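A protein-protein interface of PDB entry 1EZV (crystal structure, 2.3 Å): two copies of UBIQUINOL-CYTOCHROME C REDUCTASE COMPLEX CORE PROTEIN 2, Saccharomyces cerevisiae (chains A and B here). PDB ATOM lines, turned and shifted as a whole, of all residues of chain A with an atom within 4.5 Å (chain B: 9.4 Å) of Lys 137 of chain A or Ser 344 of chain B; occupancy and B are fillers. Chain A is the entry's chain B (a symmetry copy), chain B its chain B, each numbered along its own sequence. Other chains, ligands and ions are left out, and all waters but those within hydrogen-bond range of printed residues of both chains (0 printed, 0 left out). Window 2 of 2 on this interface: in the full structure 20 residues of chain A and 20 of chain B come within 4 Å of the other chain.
Of the printed residues of chain B, Lys 137 of chain A touches Ser 344. Of the printed residues of chain A, Arg 216 of chain B touches Asp 29 (2.8 Å). Of the printed residues of chain B, Asp 29 of chain A touches Arg 216 and Ser 344. Asn 345 of chain B touches none of the printed residues of chain A.
O of Arg 136 of chain A lies within hydrogen-bond range of OH of Tyr 348 of chain B (2.7 Å). The side-chain hydroxyl (OG) of Ser 344 of chain B lies close to the side-chain carboxylate (OD1) of Asp 29 of chain A. The guanidinium group (NH1) of Arg 216 of chain B is in salt-bridge range of the side-chain carboxylate (OD2) of Asp 29 of chain A (2.8 Å).
ND2 of Asn 141 of chain A lies within hydrogen-bond range of O of Gly 138 of chain A.
No position is printed for both chains. Of the 5 pairs that touch across the chains among the printed residues, none has its exchanged pair printed and touching as well.
Of the 7 printed residues of chain A, 4 touch a printed residue of chain B. Printed residues of chain A that touch a printed residue of chain B: Asp 29, Arg 136, Lys 137 and Asn 141. Hydrophobic or aromatic side chains of chain B within 4 Å of the printed part of chain A: Tyr 348.
Among the printed residues, pairs that only touch across the chains: Lys 137 of chain A with Ser 344 of chain B and Asn 141 of chain A with Ser 344 of chain B.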
ATOM      1  N   ASP A  29      -5.297  -7.116 -22.662  1.00  0.00           N
ATOM      2  CA  ASP A  29      -5.912  -6.013 -21.924  1.00  0.00           C
ATOM      3  C   ASP A  29      -6.363  -4.856 -22.812  1.00  0.00           C
ATOM      4  O   ASP A  29      -5.570  -4.290 -23.568  1.00  0.00           O
ATOM      5  CB  ASP A  29      -4.952  -5.496 -20.849  1.00  0.00           C
ATOM      6  CG  ASP A  29      -4.891  -6.405 -19.634  1.00  0.00           C
ATOM      7  OD1 ASP A  29      -4.962  -7.640 -19.800  1.00  0.00           O
ATOM      8  OD2 ASP A  29      -4.773  -5.885 -18.507  1.00  0.00           O
ATOM      9  N   PHE A 135     -13.646 -10.565  -8.584  1.00  0.00           N
ATOM     10  CA  PHE A 135     -13.353 -11.511  -9.662  1.00  0.00           C
ATOM     11  C   PHE A 135     -11.966 -11.217 -10.219  1.00  0.00           C
ATOM     12  O   PHE A 135     -11.795 -10.295 -11.012  1.00  0.00           O
ATOM     13  CB  PHE A 135     -14.385 -11.391 -10.787  1.00  0.00           C
ATOM     14  CG  PHE A 135     -15.682 -10.761 -10.366  1.00  0.00           C
ATOM     15  CD1 PHE A 135     -16.628 -11.487  -9.653  1.00  0.00           C
ATOM     16  CD2 PHE A 135     -15.988  -9.461 -10.746  1.00  0.00           C
ATOM     17  CE1 PHE A 135     -17.866 -10.927  -9.332  1.00  0.00           C
ATOM     18  CE2 PHE A 135     -17.224  -8.893 -10.428  1.00  0.00           C
ATOM     19  CZ  PHE A 135     -18.164  -9.630  -9.723  1.00  0.00           C
ATOM     20  N   ARG A 136     -10.988 -12.033  -9.846  1.00  0.00           N
ATOM     21  CA  ARG A 136      -9.586 -11.692 -10.069  1.00  0.00           C
ATOM     22  C   ARG A 136      -9.092 -11.709 -11.519  1.00  0.00           C
ATOM     23  O   ARG A 136      -7.991 -11.231 -11.791  1.00  0.00           O
ATOM     24  CB  ARG A 136      -8.687 -12.587  -9.212  1.00  0.00           C
ATOM     25  CG  ARG A 136      -8.435 -12.037  -7.815  1.00  0.00           C
ATOM     26  CD  ARG A 136      -8.250 -13.151  -6.798  1.00  0.00           C
ATOM     27  NE  ARG A 136      -6.848 -13.436  -6.506  1.00  0.00           N
ATOM     28  CZ  ARG A 136      -6.358 -13.584  -5.278  1.00  0.00           C
ATOM     29  NH1 ARG A 136      -5.071 -13.852  -5.102  1.00  0.00           N
ATOM     30  NH2 ARG A 136      -7.151 -13.454  -4.222  1.00  0.00           N
ATOM     31  N   LYS A 137      -9.890 -12.238 -12.446  1.00  0.00           N
ATOM     32  CA  LYS A 137      -9.445 -12.361 -13.835  1.00  0.00           C
ATOM     33  C   LYS A 137     -10.557 -12.641 -14.837  1.00  0.00           C
ATOM     34  O   LYS A 137     -10.292 -13.093 -15.951  1.00  0.00           O
ATOM     35  CB  LYS A 137      -8.375 -13.453 -13.959  1.00  0.00           C
ATOM     36  CG  LYS A 137      -7.215 -13.074 -14.869  1.00  0.00           C
ATOM     37  CD  LYS A 137      -6.356 -14.274 -15.234  1.00  0.00           C
ATOM     38  CE  LYS A 137      -5.311 -13.903 -16.281  1.00  0.00           C
ATOM     39  NZ  LYS A 137      -5.917 -13.284 -17.500  1.00  0.00           N
ATOM     40  N   GLY A 138     -11.792 -12.333 -14.460  1.00  0.00           N
ATOM     41  CA  GLY A 138     -12.910 -12.551 -15.362  1.00  0.00           C
ATOM     42  C   GLY A 138     -13.604 -11.254 -15.720  1.00  0.00           C
ATOM     43  O   GLY A 138     -13.350 -10.679 -16.779  1.00  0.00           O
ATOM     44  N   LEU A 139     -14.524 -10.832 -14.857  1.00  0.00           N
ATOM     45  CA  LEU A 139     -15.120  -9.503 -14.940  1.00  0.00           C
ATOM     46  C   LEU A 139     -14.193  -8.490 -14.271  1.00  0.00           C
ATOM     47  O   LEU A 139     -14.484  -7.294 -14.238  1.00  0.00           O
ATOM     48  CB  LEU A 139     -16.486  -9.472 -14.242  1.00  0.00           C
ATOM     49  CG  LEU A 139     -17.497 -10.591 -14.495  1.00  0.00           C
ATOM     50  CD1 LEU A 139     -17.156 -11.810 -13.646  1.00  0.00           C
ATOM     51  CD2 LEU A 139     -18.891 -10.094 -14.160  1.00  0.00           C
ATOM     52  N   ASN A 141     -11.228  -8.059 -15.341  1.00  0.00           N
ATOM     53  CA  ASN A 141     -10.377  -7.572 -16.418  1.00  0.00           C
ATOM     54  C   ASN A 141     -10.618  -6.075 -16.620  1.00  0.00           C
ATOM     55  O   ASN A 141     -11.747  -5.594 -16.479  1.00  0.00           O
ATOM     56  CB  ASN A 141     -10.674  -8.328 -17.721  1.00  0.00           C
ATOM     57  CG  ASN A 141      -9.947  -9.666 -17.812  1.00  0.00           C
ATOM     58  OD1 ASN A 141      -8.943  -9.903 -17.127  1.00  0.00           O
ATOM     59  ND2 ASN A 141     -10.428 -10.532 -18.697  1.00  0.00           N
ATOM     60  N   ARG B 214      -1.206  -5.033  -6.200  1.00  0.00           N
ATOM     61  CA  ARG B 214      -0.916  -5.114  -7.631  1.00  0.00           C
ATOM     62  C   ARG B 214      -1.039  -3.747  -8.309  1.00  0.00           C
ATOM     63  O   ARG B 214      -2.134  -3.180  -8.383  1.00  0.00           O
ATOM     64  CB  ARG B 214      -1.872  -6.102  -8.309  1.00  0.00           C
ATOM     65  CG  ARG B 214      -2.041  -7.424  -7.576  1.00  0.00           C
ATOM     66  CD  ARG B 214      -3.033  -8.328  -8.287  1.00  0.00           C
ATOM     67  NE  ARG B 214      -2.480  -8.918  -9.505  1.00  0.00           N
ATOM     68  CZ  ARG B 214      -1.483  -9.800  -9.532  1.00  0.00           C
ATOM     69  NH1 ARG B 214      -1.077 -10.301 -10.689  1.00  0.00           N
ATOM     70  NH2 ARG B 214      -0.882 -10.174  -8.411  1.00  0.00           N
ATOM     71  N   VAL B 215       0.078  -3.238  -8.825  1.00  0.00           N
ATOM     72  CA  VAL B 215       0.080  -1.958  -9.534  1.00  0.00           C
ATOM     73  C   VAL B 215       0.404  -2.127 -11.016  1.00  0.00           C
ATOM     74  O   VAL B 215       1.461  -2.654 -11.381  1.00  0.00           O
ATOM     75  CB  VAL B 215       1.098  -0.962  -8.928  1.00  0.00           C
ATOM     76  CG1 VAL B 215       0.825   0.437  -9.453  1.00  0.00           C
ATOM     77  CG2 VAL B 215       1.021  -0.982  -7.411  1.00  0.00           C
ATOM     78  N   ARG B 216      -0.503  -1.644 -11.860  1.00  0.00           N
ATOM     79  CA  ARG B 216      -0.307  -1.643 -13.307  1.00  0.00           C
ATOM     80  C   ARG B 216       0.736  -0.598 -13.696  1.00  0.00           C
ATOM     81  O   ARG B 216       0.738   0.517 -13.170  1.00  0.00           O
ATOM     82  CB  ARG B 216      -1.627  -1.343 -14.016  1.00  0.00           C
ATOM     83  CG  ARG B 216      -2.860  -1.618 -13.174  1.00  0.00           C
ATOM     84  CD  ARG B 216      -4.139  -1.388 -13.959  1.00  0.00           C
ATOM     85  NE  ARG B 216      -4.476  -2.536 -14.796  1.00  0.00           N
ATOM     86  CZ  ARG B 216      -4.073  -2.689 -16.053  1.00  0.00           C
ATOM     87  NH1 ARG B 216      -4.393  -3.783 -16.728  1.00  0.00           N
ATOM     88  NH2 ARG B 216      -3.353  -1.746 -16.639  1.00  0.00           N
ATOM     89  N   PHE B 217       1.627  -0.971 -14.609  1.00  0.00           N
ATOM     90  CA  PHE B 217       2.781  -0.143 -14.938  1.00  0.00           C
ATOM     91  C   PHE B 217       3.240  -0.403 -16.366  1.00  0.00           C
ATOM     92  O   PHE B 217       3.405  -1.553 -16.775  1.00  0.00           O
ATOM     93  CB  PHE B 217       3.926  -0.440 -13.964  1.00  0.00           C
ATOM     94  CG  PHE B 217       5.125   0.455 -14.135  1.00  0.00           C
ATOM     95  CD1 PHE B 217       5.165   1.708 -13.531  1.00  0.00           C
ATOM     96  CD2 PHE B 217       6.242   0.019 -14.845  1.00  0.00           C
ATOM     97  CE1 PHE B 217       6.302   2.512 -13.626  1.00  0.00           C
ATOM     98  CE2 PHE B 217       7.380   0.815 -14.947  1.00  0.00           C
ATOM     99  CZ  PHE B 217       7.410   2.064 -14.335  1.00  0.00           C
ATOM    100  N   SER B 221       8.341  -5.434 -15.847  1.00  0.00           N
ATOM    101  CA  SER B 221       7.548  -6.080 -14.808  1.00  0.00           C
ATOM    102  C   SER B 221       8.431  -6.518 -13.648  1.00  0.00           C
ATOM    103  O   SER B 221       9.570  -6.943 -13.848  1.00  0.00           O
ATOM    104  CB  SER B 221       6.797  -7.285 -15.375  1.00  0.00           C
ATOM    105  OG  SER B 221       5.598  -6.876 -16.010  1.00  0.00           O
ATOM    106  N   SER B 278       6.355 -10.629 -18.792  1.00  0.00           N
ATOM    107  CA  SER B 278       5.688 -11.134 -17.601  1.00  0.00           C
ATOM    108  C   SER B 278       5.854 -12.639 -17.395  1.00  0.00           C
ATOM    109  O   SER B 278       5.629 -13.146 -16.295  1.00  0.00           O
ATOM    110  CB  SER B 278       4.206 -10.787 -17.676  1.00  0.00           C
ATOM    111  OG  SER B 278       3.706 -11.030 -18.980  1.00  0.00           O
ATOM    112  N   ALA B 279       6.205 -13.351 -18.461  1.00  0.00           N
ATOM    113  CA  ALA B 279       6.395 -14.793 -18.388  1.00  0.00           C
ATOM    114  C   ALA B 279       7.633 -15.146 -17.568  1.00  0.00           C
ATOM    115  O   ALA B 279       7.584 -16.029 -16.712  1.00  0.00           O
ATOM    116  CB  ALA B 279       6.505 -15.379 -19.788  1.00  0.00           C
ATOM    117  N   SER B 282       7.042 -14.297 -13.772  1.00  0.00           N
ATOM    118  CA  SER B 282       6.179 -15.286 -13.132  1.00  0.00           C
ATOM    119  C   SER B 282       6.951 -16.530 -12.700  1.00  0.00           C
ATOM    120  O   SER B 282       6.830 -16.976 -11.562  1.00  0.00           O
ATOM    121  CB  SER B 282       5.046 -15.695 -14.077  1.00  0.00           C
ATOM    122  OG  SER B 282       4.064 -14.680 -14.176  1.00  0.00           O
ATOM    123  N   ALA B 339       2.914  -7.246  -7.106  1.00  0.00           N
ATOM    124  CA  ALA B 339       3.112  -7.363  -8.542  1.00  0.00           C
ATOM    125  C   ALA B 339       3.018  -5.983  -9.178  1.00  0.00           C
ATOM    126  O   ALA B 339       2.031  -5.264  -8.989  1.00  0.00           O
ATOM    127  CB  ALA B 339       2.064  -8.286  -9.140  1.00  0.00           C
ATOM    128  N   VAL B 340       4.091  -5.589  -9.857  1.00  0.00           N
ATOM    129  CA  VAL B 340       4.143  -4.314 -10.565  1.00  0.00           C
ATOM    130  C   VAL B 340       4.463  -4.562 -12.036  1.00  0.00           C
ATOM    131  O   VAL B 340       5.477  -5.186 -12.364  1.00  0.00           O
ATOM    132  CB  VAL B 340       5.226  -3.384  -9.965  1.00  0.00           C
ATOM    133  CG1 VAL B 340       5.281  -2.069 -10.735  1.00  0.00           C
ATOM    134  CG2 VAL B 340       4.941  -3.120  -8.494  1.00  0.00           C
ATOM    135  N   GLY B 341       3.555  -4.137 -12.910  1.00  0.00           N
ATOM    136  CA  GLY B 341       3.825  -4.181 -14.336  1.00  0.00           C
ATOM    137  C   GLY B 341       2.692  -4.779 -15.140  1.00  0.00           C
ATOM    138  O   GLY B 341       1.551  -4.323 -15.057  1.00  0.00           O
ATOM    139  N   ASP B 342       3.030  -5.766 -15.965  1.00  0.00           N
ATOM    140  CA  ASP B 342       2.046  -6.534 -16.716  1.00  0.00           C
ATOM    141  C   ASP B 342       1.251  -7.400 -15.742  1.00  0.00           C
ATOM    142  O   ASP B 342       1.536  -8.586 -15.563  1.00  0.00           O
ATOM    143  CB  ASP B 342       2.755  -7.404 -17.759  1.00  0.00           C
ATOM    144  CG  ASP B 342       1.813  -7.933 -18.828  1.00  0.00           C
ATOM    145  OD1 ASP B 342       2.312  -8.559 -19.787  1.00  0.00           O
ATOM    146  OD2 ASP B 342       0.582  -7.728 -18.722  1.00  0.00           O
ATOM    147  N   VAL B 343       0.227  -6.798 -15.146  1.00  0.00           N
ATOM    148  CA  VAL B 343      -0.422  -7.343 -13.959  1.00  0.00           C
ATOM    149  C   VAL B 343      -1.354  -8.519 -14.271  1.00  0.00           C
ATOM    150  O   VAL B 343      -1.415  -9.486 -13.508  1.00  0.00           O
ATOM    151  CB  VAL B 343      -1.165  -6.202 -13.185  1.00  0.00           C
ATOM    152  CG1 VAL B 343      -2.626  -6.560 -12.894  1.00  0.00           C
ATOM    153  CG2 VAL B 343      -0.418  -5.896 -11.900  1.00  0.00           C
ATOM    154  N   SER B 344      -1.993  -8.475 -15.437  1.00  0.00           N
ATOM    155  CA  SER B 344      -2.884  -9.546 -15.873  1.00  0.00           C
ATOM    156  C   SER B 344      -2.092 -10.781 -16.317  1.00  0.00           C
ATOM    157  O   SER B 344      -2.667 -11.773 -16.766  1.00  0.00           O
ATOM    158  CB  SER B 344      -3.769  -9.051 -17.020  1.00  0.00           C
ATOM    159  OG  SER B 344      -5.109  -9.488 -16.870  1.00  0.00           O
ATOM    160  N   ASN B 345      -0.777 -10.735 -16.123  1.00  0.00           N
ATOM    161  CA  ASN B 345       0.110 -11.819 -16.527  1.00  0.00           C
ATOM    162  C   ASN B 345       1.124 -12.136 -15.433  1.00  0.00           C
ATOM    163  O   ASN B 345       2.203 -12.666 -15.702  1.00  0.00           O
ATOM    164  CB  ASN B 345       0.849 -11.432 -17.803  1.00  0.00           C
ATOM    165  CG  ASN B 345       0.226 -12.024 -19.041  1.00  0.00           C
ATOM    166  OD1 ASN B 345       0.722 -13.013 -19.582  1.00  0.00           O
ATOM    167  ND2 ASN B 345      -0.836 -11.391 -19.532  1.00  0.00           N
ATOM    168  N   LEU B 346       0.788 -11.771 -14.203  1.00  0.00           N
ATOM    169  CA  LEU B 346       1.674 -11.993 -13.069  1.00  0.00           C
ATOM    170  C   LEU B 346       0.971 -12.825 -11.994  1.00  0.00           C
ATOM    171  O   LEU B 346      -0.261 -12.839 -11.914  1.00  0.00           O
ATOM    172  CB  LEU B 346       2.139 -10.645 -12.497  1.00  0.00           C
ATOM    173  CG  LEU B 346       3.622 -10.263 -12.631  1.00  0.00           C
ATOM    174  CD1 LEU B 346       4.206 -10.787 -13.926  1.00  0.00           C
ATOM    175  CD2 LEU B 346       3.761  -8.752 -12.570  1.00  0.00           C
ATOM    176  N   PRO B 347       1.744 -13.591 -11.206  1.00  0.00           N
ATOM    177  CA  PRO B 347       1.183 -14.455 -10.162  1.00  0.00           C
ATOM    178  C   PRO B 347       0.408 -13.675  -9.105  1.00  0.00           C
ATOM    179  O   PRO B 347       0.770 -12.551  -8.759  1.00  0.00           O
ATOM    180  CB  PRO B 347       2.416 -15.127  -9.551  1.00  0.00           C
ATOM    181  CG  PRO B 347       3.471 -15.007 -10.591  1.00  0.00           C
ATOM    182  CD  PRO B 347       3.213 -13.693 -11.252  1.00  0.00           C
ATOM    183  N   TYR B 348      -0.683 -14.263  -8.632  1.00  0.00           N
ATOM    184  CA  TYR B 348      -1.317 -13.805  -7.404  1.00  0.00           C
ATOM    185  C   TYR B 348      -0.645 -14.492  -6.217  1.00  0.00           C
ATOM    186  O   TYR B 348       0.237 -15.337  -6.399  1.00  0.00           O
ATOM    187  CB  TYR B 348      -2.815 -14.114  -7.433  1.00  0.00           C
ATOM    188  CG  TYR B 348      -3.612 -13.151  -8.287  1.00  0.00           C
ATOM    189  CD1 TYR B 348      -4.264 -12.059  -7.714  1.00  0.00           C
ATOM    190  CD2 TYR B 348      -3.685 -13.308  -9.672  1.00  0.00           C
ATOM    191  CE1 TYR B 348      -4.969 -11.146  -8.498  1.00  0.00           C
ATOM    192  CE2 TYR B 348      -4.384 -12.397 -10.466  1.00  0.00           C
ATOM    193  CZ  TYR B 348      -5.022 -11.319  -9.871  1.00  0.00           C
ATOM    194  OH  TYR B 348      -5.696 -10.404 -10.646  1.00  0.00           O
ATOM    195  N   GLU B 351      -0.802 -18.715  -5.581  1.00  0.00           N
ATOM    196  CA  GLU B 351      -0.124 -19.765  -6.336  1.00  0.00           C
ATOM    197  C   GLU B 351       1.397 -19.764  -6.181  1.00  0.00           C
ATOM    198  O   GLU B 351       2.116 -20.225  -7.071  1.00  0.00           O
ATOM    199  CB  GLU B 351      -0.500 -19.653  -7.818  1.00  0.00           C
ATOM    200  CG  GLU B 351      -0.265 -18.271  -8.419  1.00  0.00           C
ATOM    201  CD  GLU B 351      -1.008 -18.060  -9.723  1.00  0.00           C
ATOM    202  OE1 GLU B 351      -0.461 -18.427 -10.787  1.00  0.00           O
ATOM    203  OE2 GLU B 351      -2.130 -17.511  -9.685  1.00  0.00           O
